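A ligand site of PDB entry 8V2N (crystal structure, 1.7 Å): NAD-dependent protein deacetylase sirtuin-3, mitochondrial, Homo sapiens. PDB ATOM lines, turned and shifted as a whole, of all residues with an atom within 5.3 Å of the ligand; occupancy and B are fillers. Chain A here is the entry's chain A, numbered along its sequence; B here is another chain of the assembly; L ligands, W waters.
The backbone NH (N) of Arg 228 sits at hydrogen-bond distance from a nitrogen (N5) of the ligand, at 3.0 Å. N of Ala 29 sits at hydrogen-bond distance from O8 of the ligand (2.8 Å). The backbone NH of Ile 113 lies within hydrogen-bond range of an oxygen (O13) of the ligand. The side-chain amide nitrogen of Gln 111 lies within hydrogen-bond range of an oxygen (O8) of the ligand. The side-chain hydroxyl of Ser 204 is in hydrogen-bond range of an oxygen (O1) of the ligand (2.8 Å). A nitrogen (N4) of the ligand lies within hydrogen-bond range of the backbone NH of Val 249, at 2.8 Å. A nitrogen (N7) of the ligand sits at hydrogen-bond distance from the side-chain carboxylate of Asp 114 (2.8 Å). The backbone NH (N) of Ser 204 sits at hydrogen-bond distance from an oxygen (O9) of the ligand (2.8 Å). OAY of FDL 4 of chain B sits at hydrogen-bond distance from O11 of the ligand, at 2.5 Å. The side-chain amide nitrogen of Asn 227 is in hydrogen-bond range of an oxygen (O5) of the ligand, at 3.2 Å. An oxygen (O13) of the ligand lies within hydrogen-bond range of the backbone NH (N) of Asp 114. The side-chain hydroxyl (OG1) of Thr 33 is in hydrogen-bond range of a nitrogen (N2) of the ligand (3.0 Å). A nitrogen (N2) of the ligand lies close to the guanidinium group (NH1) of Arg 228 (3.4 Å). The side-chain carboxylate of Asp 248 is in hydrogen-bond range of a nitrogen (N3) of the ligand, 2.9 Å away. The side-chain hydroxyl (OG1) of Thr 203 sits at hydrogen-bond distance from an oxygen (O9) of the ligand (3.0 Å). The backbone NH (N) of Phe 40 lies within hydrogen-bond range of an oxygen (O2) of the ligand (3.0 Å). An oxygen (O2) of the ligand lies within hydrogen-bond range of the backbone NH (N) of Arg 41 (2.7 Å).
N of Gln 111 lies within hydrogen-bond range of O of Val 27, 3.1 Å away. The side-chain amide nitrogen (ND2) of Asn 112 is in hydrogen-bond range of the backbone carbonyl oxygen (O) of Gly 28, 2.9 Å away. OD2 of Asp 248 sits at hydrogen-bond distance from N of Val 250 (2.8 Å). The backbone NH (N) of Thr 203 is in hydrogen-bond range of the side-chain amide oxygen (OD1) of Asn 227 (3.3 Å). The backbone NH of Ile 37 lies within hydrogen-bond range of the backbone carbonyl oxygen of Ser 32, 3.2 Å away. O of Phe 63 is in hydrogen-bond range of N of Phe 177, 2.8 Å away. The side-chain hydroxyl (OG1) of Thr 33 is in hydrogen-bond range of the backbone carbonyl oxygen (O) of Gly 30 (3.1 Å). The side-chain hydroxyl (OG1) of Thr 203 sits at hydrogen-bond distance from the side-chain amide nitrogen (NE2) of Gln 111, 3.0 Å away.
The backbone carbonyl oxygen of Gly 202 lies close to an oxygen (O4) of the ligand (3.5 Å). Residues that only touch the ligand: Gly 28, Gly 30, Ser 32, Ile 37, Pro 38, Asp 39, Phe 63, Asn 112, His 131, Leu 205, Val 207 and Gly 247. 27 residues have an atom within 4 Å of the ligand: Gly 28, Ala 29, Gly 30, Ser 32, Thr 33, Ile 37, Pro 38, Asp 39, Phe 40, Arg 41, Phe 63, Gln 111, Asn 112, Ile 113, Asp 114, His 131, Gly 202, Thr 203, Ser 204, Leu 205, Val 207, Asn 227, Arg 228, Gly 247, Asp 248, Val 249 and FDL 4 of chain B. The nearest printed residue that does not touch the ligand is Val 231 (4.3 Å).
Water W2 lies within hydrogen-bond range of O of Ala 29 (2.8 Å), O of Ile 37 (2.8 Å) and N7 of the ligand (2.9 Å).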
ATOM      1  N   VAL A  27      -9.889 -27.318  -8.123  1.00  0.00           N
ATOM      2  CA  VAL A  27      -8.677 -26.492  -8.098  1.00  0.00           C
ATOM      3  C   VAL A  27      -7.450 -27.372  -7.997  1.00  0.00           C
ATOM      4  O   VAL A  27      -7.501 -28.480  -7.420  1.00  0.00           O
ATOM      5  CB  VAL A  27      -8.696 -25.436  -6.996  1.00  0.00           C
ATOM      6  CG1 VAL A  27      -9.923 -24.555  -7.097  1.00  0.00           C
ATOM      7  CG2 VAL A  27      -8.565 -26.023  -5.582  1.00  0.00           C
ATOM      8  N   GLY A  28      -6.342 -26.784  -8.396  1.00  0.00           N
ATOM      9  CA  GLY A  28      -5.031 -27.398  -8.299  1.00  0.00           C
ATOM     10  C   GLY A  28      -4.006 -26.359  -7.892  1.00  0.00           C
ATOM     11  O   GLY A  28      -4.374 -25.294  -7.425  1.00  0.00           O
ATOM     12  N   ALA A  29      -2.734 -26.647  -8.166  1.00  0.00           N
ATOM     13  CA  ALA A  29      -1.627 -25.912  -7.561  1.00  0.00           C
ATOM     14  C   ALA A  29      -1.545 -24.509  -8.165  1.00  0.00           C
ATOM     15  O   ALA A  29      -0.916 -23.607  -7.584  1.00  0.00           O
ATOM     16  CB  ALA A  29      -0.337 -26.697  -7.782  1.00  0.00           C
ATOM     17  N   GLY A  30      -2.125 -24.343  -9.360  1.00  0.00           N
ATOM     18  CA  GLY A  30      -2.203 -23.054 -10.009  1.00  0.00           C
ATOM     19  C   GLY A  30      -2.769 -21.972  -9.078  1.00  0.00           C
ATOM     20  O   GLY A  30      -2.289 -20.840  -9.087  1.00  0.00           O
ATOM     21  N   SER A  32      -2.467 -21.661  -6.038  1.00  0.00           N
ATOM     22  CA  SER A  32      -1.658 -21.402  -4.850  1.00  0.00           C
ATOM     23  C   SER A  32      -0.290 -20.854  -5.214  1.00  0.00           C
ATOM     24  O   SER A  32       0.467 -20.499  -4.327  1.00  0.00           O
ATOM     25  CB  SER A  32      -1.577 -22.600  -3.962  1.00  0.00           C
ATOM     26  OG  SER A  32      -2.789 -22.766  -3.260  1.00  0.00           O
ATOM     27  N   THR A  33      -0.016 -20.674  -6.517  1.00  0.00           N
ATOM     28  CA  THR A  33       1.252 -20.059  -6.925  1.00  0.00           C
ATOM     29  C   THR A  33       1.229 -18.564  -6.612  1.00  0.00           C
ATOM     30  O   THR A  33       2.281 -17.976  -6.321  1.00  0.00           O
ATOM     31  CB  THR A  33       1.635 -20.407  -8.365  1.00  0.00           C
ATOM     32  OG1 THR A  33       0.662 -19.863  -9.262  1.00  0.00           O
ATOM     33  CG2 THR A  33       1.812 -21.895  -8.584  1.00  0.00           C
ATOM     34  N   PRO A  34       0.046 -17.899  -6.617  1.00  0.00           N
ATOM     35  CA  PRO A  34      -0.050 -16.508  -6.177  1.00  0.00           C
ATOM     36  C   PRO A  34       0.292 -16.342  -4.689  1.00  0.00           C
ATOM     37  O   PRO A  34       0.631 -15.245  -4.232  1.00  0.00           O
ATOM     38  CB  PRO A  34      -1.534 -16.159  -6.426  1.00  0.00           C
ATOM     39  CG  PRO A  34      -1.977 -17.179  -7.473  1.00  0.00           C
ATOM     40  CD  PRO A  34      -1.223 -18.433  -7.130  1.00  0.00           C
ATOM     41  N   ILE A  37       3.544 -20.547  -3.332  1.00  0.00           N
ATOM     42  CA  ILE A  37       3.823 -21.975  -3.419  1.00  0.00           C
ATOM     43  C   ILE A  37       3.981 -22.346  -4.890  1.00  0.00           C
ATOM     44  O   ILE A  37       3.006 -22.331  -5.646  1.00  0.00           O
ATOM     45  CB  ILE A  37       2.701 -22.803  -2.759  1.00  0.00           C
ATOM     46  CG1 ILE A  37       2.458 -22.365  -1.323  1.00  0.00           C
ATOM     47  CG2 ILE A  37       3.002 -24.304  -2.865  1.00  0.00           C
ATOM     48  CD1 ILE A  37       1.161 -22.849  -0.753  1.00  0.00           C
ATOM     49  N   PRO A  38       5.193 -22.755  -5.316  1.00  0.00           N
ATOM     50  CA  PRO A  38       5.409 -23.202  -6.686  1.00  0.00           C
ATOM     51  C   PRO A  38       4.567 -24.447  -6.975  1.00  0.00           C
ATOM     52  O   PRO A  38       4.407 -25.309  -6.116  1.00  0.00           O
ATOM     53  CB  PRO A  38       6.910 -23.566  -6.738  1.00  0.00           C
ATOM     54  CG  PRO A  38       7.510 -22.915  -5.487  1.00  0.00           C
ATOM     55  CD  PRO A  38       6.382 -22.902  -4.476  1.00  0.00           C
ATOM     56  N   ASP A  39       4.010 -24.515  -8.194  1.00  0.00           N
ATOM     57  CA  ASP A  39       3.319 -25.698  -8.661  1.00  0.00           C
ATOM     58  C   ASP A  39       4.345 -26.758  -9.096  1.00  0.00           C
ATOM     59  O   ASP A  39       5.559 -26.567  -8.915  1.00  0.00           O
ATOM     60  CB  ASP A  39       2.326 -25.359  -9.792  1.00  0.00           C
ATOM     61  CG  ASP A  39       2.980 -24.733 -11.001  1.00  0.00           C
ATOM     62  OD1 ASP A  39       4.160 -25.110 -11.312  1.00  0.00           O
ATOM     63  OD2 ASP A  39       2.339 -23.874 -11.639  1.00  0.00           O
ATOM     64  N   PHE A  40       3.853 -27.868  -9.670  1.00  0.00           N
ATOM     65  CA  PHE A  40       4.699 -28.866 -10.309  1.00  0.00           C
ATOM     66  C   PHE A  40       4.844 -28.528 -11.800  1.00  0.00           C
ATOM     67  O   PHE A  40       5.938 -28.576 -12.354  1.00  0.00           O
ATOM     68  CB  PHE A  40       4.117 -30.278 -10.134  1.00  0.00           C
ATOM     69  CG  PHE A  40       4.381 -30.942  -8.794  1.00  0.00           C
ATOM     70  CD1 PHE A  40       5.166 -30.327  -7.828  1.00  0.00           C
ATOM     71  CD2 PHE A  40       3.861 -32.196  -8.519  1.00  0.00           C
ATOM     72  CE1 PHE A  40       5.409 -30.947  -6.608  1.00  0.00           C
ATOM     73  CE2 PHE A  40       4.103 -32.816  -7.299  1.00  0.00           C
ATOM     74  CZ  PHE A  40       4.876 -32.190  -6.348  1.00  0.00           C
ATOM     75  N   ARG A  41       3.701 -28.219 -12.461  1.00  0.00           N
ATOM     76  CA  ARG A  41       3.658 -28.021 -13.904  1.00  0.00           C
ATOM     77  C   ARG A  41       3.792 -26.535 -14.228  1.00  0.00           C
ATOM     78  O   ARG A  41       4.931 -26.106 -14.464  1.00  0.00           O
ATOM     79  CB  ARG A  41       2.364 -28.605 -14.495  1.00  0.00           C
ATOM     80  N   PHE A  63       5.870 -38.748  -3.405  1.00  0.00           N
ATOM     81  CA  PHE A  63       4.579 -39.265  -2.924  1.00  0.00           C
ATOM     82  C   PHE A  63       4.488 -40.772  -3.166  1.00  0.00           C
ATOM     83  O   PHE A  63       3.399 -41.293  -3.373  1.00  0.00           O
ATOM     84  CB  PHE A  63       3.412 -38.541  -3.591  1.00  0.00           C
ATOM     85  CG  PHE A  63       3.404 -37.060  -3.373  1.00  0.00           C
ATOM     86  CD1 PHE A  63       3.660 -36.528  -2.124  1.00  0.00           C
ATOM     87  CD2 PHE A  63       3.141 -36.191  -4.433  1.00  0.00           C
ATOM     88  CE1 PHE A  63       3.640 -35.158  -1.922  1.00  0.00           C
ATOM     89  CE2 PHE A  63       3.121 -34.821  -4.232  1.00  0.00           C
ATOM     90  CZ  PHE A  63       3.395 -34.302  -2.980  1.00  0.00           C
ATOM     91  N   LEU A  82       5.513 -26.614   3.316  1.00  0.00           N
ATOM     92  CA  LEU A  82       4.110 -26.540   2.942  1.00  0.00           C
ATOM     93  C   LEU A  82       3.237 -26.371   4.169  1.00  0.00           C
ATOM     94  O   LEU A  82       2.062 -26.042   4.040  1.00  0.00           O
ATOM     95  CB  LEU A  82       3.725 -27.799   2.154  1.00  0.00           C
ATOM     96  CG  LEU A  82       3.867 -27.676   0.638  1.00  0.00           C
ATOM     97  CD1 LEU A  82       3.264 -28.865  -0.063  1.00  0.00           C
ATOM     98  CD2 LEU A  82       3.249 -26.382   0.144  1.00  0.00           C
ATOM     99  N   GLN A 111      -6.915 -30.608  -5.301  1.00  0.00           N
ATOM    100  CA  GLN A 111      -5.763 -31.510  -5.356  1.00  0.00           C
ATOM    101  C   GLN A 111      -4.641 -31.000  -4.468  1.00  0.00           C
ATOM    102  O   GLN A 111      -3.594 -31.653  -4.327  1.00  0.00           O
ATOM    103  CB  GLN A 111      -5.250 -31.621  -6.765  1.00  0.00           C
ATOM    104  CG  GLN A 111      -6.277 -32.112  -7.750  1.00  0.00           C
ATOM    105  CD  GLN A 111      -5.844 -31.845  -9.158  1.00  0.00           C
ATOM    106  OE1 GLN A 111      -5.238 -32.695  -9.817  1.00  0.00           O
ATOM    107  NE2 GLN A 111      -6.106 -30.631  -9.628  1.00  0.00           N
ATOM    108  N   ASN A 112      -4.829 -29.795  -3.918  1.00  0.00           N
ATOM    109  CA  ASN A 112      -3.760 -29.133  -3.203  1.00  0.00           C
ATOM    110  C   ASN A 112      -3.649 -29.738  -1.813  1.00  0.00           C
ATOM    111  O   ASN A 112      -4.637 -30.203  -1.240  1.00  0.00           O
ATOM    112  CB  ASN A 112      -3.969 -27.627  -3.122  1.00  0.00           C
ATOM    113  CG  ASN A 112      -3.983 -26.984  -4.484  1.00  0.00           C
ATOM    114  OD1 ASN A 112      -3.422 -27.512  -5.428  1.00  0.00           O
ATOM    115  ND2 ASN A 112      -4.725 -25.913  -4.616  1.00  0.00           N
ATOM    116  N   ILE A 113      -2.433 -29.687  -1.261  1.00  0.00           N
ATOM    117  CA  ILE A 113      -2.225 -30.199   0.080  1.00  0.00           C
ATOM    118  C   ILE A 113      -1.737 -29.061   0.968  1.00  0.00           C
ATOM    119  O   ILE A 113      -1.333 -29.278   2.110  1.00  0.00           O
ATOM    120  CB  ILE A 113      -1.239 -31.380   0.062  1.00  0.00           C
ATOM    121  CG1 ILE A 113       0.110 -30.965  -0.521  1.00  0.00           C
ATOM    122  CG2 ILE A 113      -1.842 -32.566  -0.704  1.00  0.00           C
ATOM    123  CD1 ILE A 113       1.182 -32.031  -0.437  1.00  0.00           C
ATOM    124  N   ASP A 114      -1.848 -27.828   0.444  1.00  0.00           N
ATOM    125  CA  ASP A 114      -1.364 -26.656   1.150  1.00  0.00           C
ATOM    126  C   ASP A 114      -2.380 -26.223   2.208  1.00  0.00           C
ATOM    127  O   ASP A 114      -2.044 -25.511   3.141  1.00  0.00           O
ATOM    128  CB  ASP A 114      -0.984 -25.534   0.172  1.00  0.00           C
ATOM    129  CG  ASP A 114      -2.161 -25.069  -0.684  1.00  0.00           C
ATOM    130  OD1 ASP A 114      -3.314 -25.061  -0.156  1.00  0.00           O
ATOM    131  OD2 ASP A 114      -1.925 -24.714  -1.883  1.00  0.00           O
ATOM    132  N   HIS A 131      -6.313 -35.022  -1.968  1.00  0.00           N
ATOM    133  CA  HIS A 131      -4.986 -35.572  -1.775  1.00  0.00           C
ATOM    134  C   HIS A 131      -4.544 -35.468  -0.316  1.00  0.00           C
ATOM    135  O   HIS A 131      -3.360 -35.634  -0.011  1.00  0.00           O
ATOM    136  CB  HIS A 131      -3.984 -34.968  -2.765  1.00  0.00           C
ATOM    137  CG  HIS A 131      -4.274 -35.327  -4.171  1.00  0.00           C
ATOM    138  ND1 HIS A 131      -3.826 -34.566  -5.239  1.00  0.00           N
ATOM    139  CD2 HIS A 131      -5.012 -36.337  -4.707  1.00  0.00           C
ATOM    140  CE1 HIS A 131      -4.236 -35.107  -6.366  1.00  0.00           C
ATOM    141  NE2 HIS A 131      -4.986 -36.181  -6.070  1.00  0.00           N
ATOM    142  N   PHE A 177       0.723 -41.868  -3.912  1.00  0.00           N
ATOM    143  CA  PHE A 177       0.422 -42.600  -5.129  1.00  0.00           C
ATOM    144  C   PHE A 177       0.073 -44.058  -4.765  1.00  0.00           C
ATOM    145  O   PHE A 177       0.736 -44.670  -3.922  1.00  0.00           O
ATOM    146  CB  PHE A 177       1.576 -42.498  -6.124  1.00  0.00           C
ATOM    147  CG  PHE A 177       1.820 -41.118  -6.692  1.00  0.00           C
ATOM    148  CD1 PHE A 177       0.771 -40.398  -7.273  1.00  0.00           C
ATOM    149  CD2 PHE A 177       3.068 -40.534  -6.643  1.00  0.00           C
ATOM    150  CE1 PHE A 177       0.994 -39.117  -7.776  1.00  0.00           C
ATOM    151  CE2 PHE A 177       3.283 -39.268  -7.171  1.00  0.00           C
ATOM    152  CZ  PHE A 177       2.246 -38.550  -7.723  1.00  0.00           C
ATOM    153  N   GLY A 202      -6.706 -23.507 -12.135  1.00  0.00           N
ATOM    154  CA  GLY A 202      -5.303 -23.746 -11.853  1.00  0.00           C
ATOM    155  C   GLY A 202      -4.978 -25.231 -11.677  1.00  0.00           C
ATOM    156  O   GLY A 202      -4.324 -25.622 -10.697  1.00  0.00           O
ATOM    157  N   THR A 203      -5.453 -26.033 -12.607  1.00  0.00           N
ATOM    158  CA  THR A 203      -5.113 -27.447 -12.623  1.00  0.00           C
ATOM    159  C   THR A 203      -4.691 -27.856 -14.028  1.00  0.00           C
ATOM    160  O   THR A 203      -5.249 -27.372 -15.002  1.00  0.00           O
ATOM    161  CB  THR A 203      -6.248 -28.325 -12.076  1.00  0.00           C
ATOM    162  OG1 THR A 203      -5.944 -29.668 -12.439  1.00  0.00           O
ATOM    163  CG2 THR A 203      -7.602 -27.936 -12.615  1.00  0.00           C
ATOM    164  N   SER A 204      -3.672 -28.699 -14.101  1.00  0.00           N
ATOM    165  CA  SER A 204      -3.219 -29.212 -15.366  1.00  0.00           C
ATOM    166  C   SER A 204      -4.130 -30.347 -15.807  1.00  0.00           C
ATOM    167  O   SER A 204      -4.129 -30.727 -16.983  1.00  0.00           O
ATOM    168  CB  SER A 204      -1.776 -29.642 -15.280  1.00  0.00           C
ATOM    169  OG  SER A 204      -1.625 -30.680 -14.336  1.00  0.00           O
ATOM    170  N   LEU A 205      -4.956 -30.841 -14.853  1.00  0.00           N
ATOM    171  CA  LEU A 205      -5.811 -32.014 -15.038  1.00  0.00           C
ATOM    172  C   LEU A 205      -4.989 -33.200 -15.546  1.00  0.00           C
ATOM    173  O   LEU A 205      -5.394 -33.873 -16.495  1.00  0.00           O
ATOM    174  CB  LEU A 205      -6.944 -31.699 -16.022  1.00  0.00           C
ATOM    175  CG  LEU A 205      -7.978 -30.689 -15.560  1.00  0.00           C
ATOM    176  CD1 LEU A 205      -9.003 -30.429 -16.682  1.00  0.00           C
ATOM    177  CD2 LEU A 205      -8.669 -31.164 -14.300  1.00  0.00           C
ATOM    178  N   GLU A 206      -3.869 -33.470 -14.878  1.00  0.00           N
ATOM    179  CA  GLU A 206      -3.040 -34.594 -15.246  1.00  0.00           C
ATOM    180  C   GLU A 206      -3.224 -35.734 -14.246  1.00  0.00           C
ATOM    181  O   GLU A 206      -2.916 -36.881 -14.559  1.00  0.00           O
ATOM    182  CB  GLU A 206      -1.583 -34.166 -15.368  1.00  0.00           C
ATOM    183  CG  GLU A 206      -1.288 -33.478 -16.673  1.00  0.00           C
ATOM    184  CD  GLU A 206      -0.018 -32.638 -16.675  1.00  0.00           C
ATOM    185  OE1 GLU A 206       0.124 -31.812 -17.588  1.00  0.00           O
ATOM    186  OE2 GLU A 206       0.822 -32.819 -15.761  1.00  0.00           O
ATOM    187  N   VAL A 207      -3.701 -35.398 -13.053  1.00  0.00           N
ATOM    188  CA  VAL A 207      -3.660 -36.333 -11.954  1.00  0.00           C
ATOM    189  C   VAL A 207      -5.027 -37.022 -11.836  1.00  0.00           C
ATOM    190  O   VAL A 207      -6.018 -36.387 -11.443  1.00  0.00           O
ATOM    191  CB  VAL A 207      -3.198 -35.661 -10.648  1.00  0.00           C
ATOM    192  CG1 VAL A 207      -3.184 -36.632  -9.472  1.00  0.00           C
ATOM    193  CG2 VAL A 207      -1.832 -35.012 -10.803  1.00  0.00           C
ATOM    194  N   ASN A 227      -7.233 -20.719 -16.162  1.00  0.00           N
ATOM    195  CA  ASN A 227      -5.980 -21.433 -16.156  1.00  0.00           C
ATOM    196  C   ASN A 227      -5.040 -20.795 -17.165  1.00  0.00           C
ATOM    197  O   ASN A 227      -5.482 -20.095 -18.081  1.00  0.00           O
ATOM    198  CB  ASN A 227      -6.171 -22.904 -16.517  1.00  0.00           C
ATOM    199  CG  ASN A 227      -5.015 -23.769 -16.063  1.00  0.00           C
ATOM    200  OD1 ASN A 227      -4.660 -23.759 -14.893  1.00  0.00           O
ATOM    201  ND2 ASN A 227      -4.369 -24.442 -17.010  1.00  0.00           N
ATOM    202  N   ARG A 228      -3.742 -21.076 -17.020  1.00  0.00           N
ATOM    203  CA  ARG A 228      -2.758 -20.604 -17.979  1.00  0.00           C
ATOM    204  C   ARG A 228      -3.115 -21.105 -19.371  1.00  0.00           C
ATOM    205  O   ARG A 228      -2.902 -20.401 -20.352  1.00  0.00           O
ATOM    206  CB  ARG A 228      -1.356 -21.069 -17.574  1.00  0.00           C
ATOM    207  CG  ARG A 228      -0.234 -20.188 -18.096  1.00  0.00           C
ATOM    208  CD  ARG A 228       1.065 -20.403 -17.344  1.00  0.00           C
ATOM    209  NE  ARG A 228       1.174 -19.599 -16.130  1.00  0.00           N
ATOM    210  CZ  ARG A 228       1.928 -19.915 -15.077  1.00  0.00           C
ATOM    211  NH1 ARG A 228       1.965 -19.121 -14.027  1.00  0.00           N
ATOM    212  NH2 ARG A 228       2.619 -21.044 -15.076  1.00  0.00           N
ATOM    213  N   VAL A 231      -6.611 -27.321 -20.901  1.00  0.00           N
ATOM    214  CA  VAL A 231      -6.029 -28.546 -20.386  1.00  0.00           C
ATOM    215  C   VAL A 231      -7.053 -29.672 -20.479  1.00  0.00           C
ATOM    216  O   VAL A 231      -8.256 -29.437 -20.443  1.00  0.00           O
ATOM    217  CB  VAL A 231      -5.502 -28.374 -18.940  1.00  0.00           C
ATOM    218  CG1 VAL A 231      -4.266 -27.485 -18.886  1.00  0.00           C
ATOM    219  CG2 VAL A 231      -6.587 -27.852 -17.999  1.00  0.00           C
ATOM    220  N   GLY A 247      -4.897 -17.260 -18.871  1.00  0.00           N
ATOM    221  CA  GLY A 247      -4.047 -16.228 -18.337  1.00  0.00           C
ATOM    222  C   GLY A 247      -3.724 -16.499 -16.886  1.00  0.00           C
ATOM    223  O   GLY A 247      -4.021 -17.582 -16.373  1.00  0.00           O
ATOM    224  N   ASP A 248      -3.198 -15.488 -16.203  1.00  0.00           N
ATOM    225  CA  ASP A 248      -2.972 -15.634 -14.785  1.00  0.00           C
ATOM    226  C   ASP A 248      -4.323 -15.871 -14.105  1.00  0.00           C
ATOM    227  O   ASP A 248      -5.326 -15.248 -14.460  1.00  0.00           O
ATOM    228  CB  ASP A 248      -2.235 -14.438 -14.192  1.00  0.00           C
ATOM    229  CG  ASP A 248      -1.942 -14.631 -12.718  1.00  0.00           C
ATOM    230  OD1 ASP A 248      -0.967 -15.338 -12.399  1.00  0.00           O
ATOM    231  OD2 ASP A 248      -2.733 -14.147 -11.910  1.00  0.00           O
ATOM    232  N   VAL A 249      -4.315 -16.778 -13.131  1.00  0.00           N
ATOM    233  CA  VAL A 249      -5.545 -17.196 -12.463  1.00  0.00           C
ATOM    234  C   VAL A 249      -6.107 -16.009 -11.678  1.00  0.00           C
ATOM    235  O   VAL A 249      -7.322 -15.845 -11.568  1.00  0.00           O
ATOM    236  CB  VAL A 249      -5.301 -18.427 -11.553  1.00  0.00           C
ATOM    237  CG1 VAL A 249      -4.415 -18.088 -10.350  1.00  0.00           C
ATOM    238  CG2 VAL A 249      -6.611 -19.070 -11.115  1.00  0.00           C
ATOM    239  N   VAL A 250      -5.219 -15.188 -11.099  1.00  0.00           N
ATOM    240  CA  VAL A 250      -5.667 -14.044 -10.307  1.00  0.00           C
ATOM    241  C   VAL A 250      -6.318 -13.012 -11.226  1.00  0.00           C
ATOM    242  O   VAL A 250      -7.319 -12.402 -10.852  1.00  0.00           O
ATOM    243  CB  VAL A 250      -4.530 -13.433  -9.472  1.00  0.00           C
ATOM    244  CG1 VAL A 250      -4.975 -12.140  -8.799  1.00  0.00           C
ATOM    245  CG2 VAL A 250      -4.024 -14.427  -8.447  1.00  0.00           C
ATOM    246  CAL FDL B   4       2.150 -42.674 -11.998  1.00  0.00           C
ATOM    247  CAD FDL B   4       1.293 -41.485 -11.612  1.00  0.00           C
ATOM    248  CAC FDL B   4       1.685 -40.191 -11.989  1.00  0.00           C
ATOM    249  CAB FDL B   4       0.897 -39.091 -11.637  1.00  0.00           C
ATOM    250  OAK FDL B   4       1.262 -37.831 -12.000  1.00  0.00           O
ATOM    251  OAA FDL B   4      -0.259 -39.275 -10.920  1.00  0.00           O
ATOM    252  CAF FDL B   4      -0.666 -40.525 -10.523  1.00  0.00           C
ATOM    253  CAG FDL B   4      -1.837 -40.665  -9.787  1.00  0.00           C
ATOM    254  CAE FDL B   4       0.109 -41.656 -10.863  1.00  0.00           C
ATOM    255  CAH FDL B   4      -0.325 -42.950 -10.467  1.00  0.00           C
ATOM    256  CAI FDL B   4      -1.502 -43.089  -9.718  1.00  0.00           C
ATOM    257  CAJ FDL B   4      -2.273 -41.946  -9.386  1.00  0.00           C
ATOM    258  NAM FDL B   4      -3.415 -42.056  -8.655  1.00  0.00           N
ATOM    259  C   FDL B   4      -3.361 -42.505  -7.392  1.00  0.00           C
ATOM    260  O   FDL B   4      -2.476 -43.256  -6.986  1.00  0.00           O
ATOM    261  CA  FDL B   4      -4.441 -42.037  -6.450  1.00  0.00           C
ATOM    262  N   FDL B   4      -5.050 -43.142  -5.759  1.00  0.00           N
ATOM    263  CB  FDL B   4      -3.851 -41.135  -5.386  1.00  0.00           C
ATOM    264  CAS FDL B   4      -2.921 -40.064  -5.933  1.00  0.00           C
ATOM    265  CAT FDL B   4      -2.419 -39.214  -4.764  1.00  0.00           C
ATOM    266  CAU FDL B   4      -1.542 -38.056  -5.205  1.00  0.00           C
ATOM    267  NAV FDL B   4      -1.151 -37.299  -4.049  1.00  0.00           N
ATOM    268  CAW FDL B   4      -0.508 -36.131  -4.108  1.00  0.00           C
ATOM    269  OAY FDL B   4      -0.405 -35.483  -5.155  1.00  0.00           O
ATOM    270  CAX FDL B   4       0.052 -35.628  -2.796  1.00  0.00           C
HETATM  271  P1  LIG L   1       0.099 -28.932 -11.692  1.00  0.00           P
HETATM  272  O1  LIG L   1       0.230 -30.274 -12.336  1.00  0.00           O
HETATM  273  O2  LIG L   1       1.328 -28.239 -11.211  1.00  0.00           O
HETATM  274  O3  LIG L   1      -0.718 -27.966 -12.680  1.00  0.00           O
HETATM  275  C1  LIG L   1      -1.091 -26.641 -12.246  1.00  0.00           C
HETATM  276  C2  LIG L   1      -1.740 -25.904 -13.392  1.00  0.00           C
HETATM  277  O4  LIG L   1      -1.963 -24.522 -13.009  1.00  0.00           O
HETATM  278  C3  LIG L   1      -0.915 -25.835 -14.696  1.00  0.00           C
HETATM  279  O5  LIG L   1      -1.769 -25.878 -15.830  1.00  0.00           O
HETATM  280  C4  LIG L   1      -0.253 -24.460 -14.586  1.00  0.00           C
HETATM  281  O6  LIG L   1       0.082 -23.889 -15.832  1.00  0.00           O
HETATM  282  C5  LIG L   1      -1.388 -23.668 -13.959  1.00  0.00           C
HETATM  283  N1  LIG L   1      -0.964 -22.443 -13.298  1.00  0.00           N
HETATM  284  C6  LIG L   1       0.032 -22.316 -12.365  1.00  0.00           C
HETATM  285  N2  LIG L   1       0.138 -21.095 -11.906  1.00  0.00           N
HETATM  286  C7  LIG L   1      -0.833 -20.370 -12.576  1.00  0.00           C
HETATM  287  C8  LIG L   1      -1.212 -19.025 -12.523  1.00  0.00           C
HETATM  288  N3  LIG L   1      -0.672 -18.133 -11.691  1.00  0.00           N
HETATM  289  N4  LIG L   1      -2.224 -18.624 -13.335  1.00  0.00           N
HETATM  290  C9  LIG L   1      -2.799 -19.535 -14.135  1.00  0.00           C
HETATM  291  N5  LIG L   1      -2.533 -20.835 -14.259  1.00  0.00           N
HETATM  292  C10 LIG L   1      -1.535 -21.203 -13.442  1.00  0.00           C
HETATM  293  O7  LIG L   1      -0.929 -29.037 -10.472  1.00  0.00           O
HETATM  294  P2  LIG L   1      -2.322 -29.825 -10.331  1.00  0.00           P
HETATM  295  O8  LIG L   1      -3.029 -29.310  -9.117  1.00  0.00           O
HETATM  296  O9  LIG L   1      -3.010 -29.779 -11.646  1.00  0.00           O
HETATM  297  O10 LIG L   1      -1.816 -31.334 -10.068  1.00  0.00           O
HETATM  298  C11 LIG L   1      -2.011 -31.960  -8.791  1.00  0.00           C
HETATM  299  C12 LIG L   1      -0.637 -32.336  -8.316  1.00  0.00           C
HETATM  300  C13 LIG L   1       0.239 -31.077  -8.083  1.00  0.00           C
HETATM  301  C14 LIG L   1      -0.616 -33.079  -6.971  1.00  0.00           C
HETATM  302  O11 LIG L   1       0.477 -33.990  -6.975  1.00  0.00           O
HETATM  303  C15 LIG L   1      -0.350 -31.965  -5.954  1.00  0.00           C
HETATM  304  O12 LIG L   1       0.042 -32.454  -4.682  1.00  0.00           O
HETATM  305  C16 LIG L   1       0.777 -31.244  -6.654  1.00  0.00           C
HETATM  306  N6  LIG L   1       1.148 -29.956  -6.004  1.00  0.00           N
HETATM  307  C17 LIG L   1       0.366 -29.343  -5.031  1.00  0.00           C
HETATM  308  C18 LIG L   1       0.784 -28.111  -4.486  1.00  0.00           C
HETATM  309  C19 LIG L   1      -0.095 -27.394  -3.511  1.00  0.00           C
HETATM  310  O13 LIG L   1      -0.719 -28.025  -2.676  1.00  0.00           O
HETATM  311  N7  LIG L   1      -0.124 -26.067  -3.572  1.00  0.00           N
HETATM  312  C20 LIG L   1       2.008 -27.600  -4.848  1.00  0.00           C
HETATM  313  C21 LIG L   1       2.673 -28.130  -5.930  1.00  0.00           C
HETATM  314  C22 LIG L   1       2.318 -29.377  -6.385  1.00  0.00           C
HETATM  315  O   HOH W   1       2.235 -32.119 -11.347  1.00  0.00           O
HETATM  316  O   HOH W   2       0.917 -24.261  -5.556  1.00  0.00           O
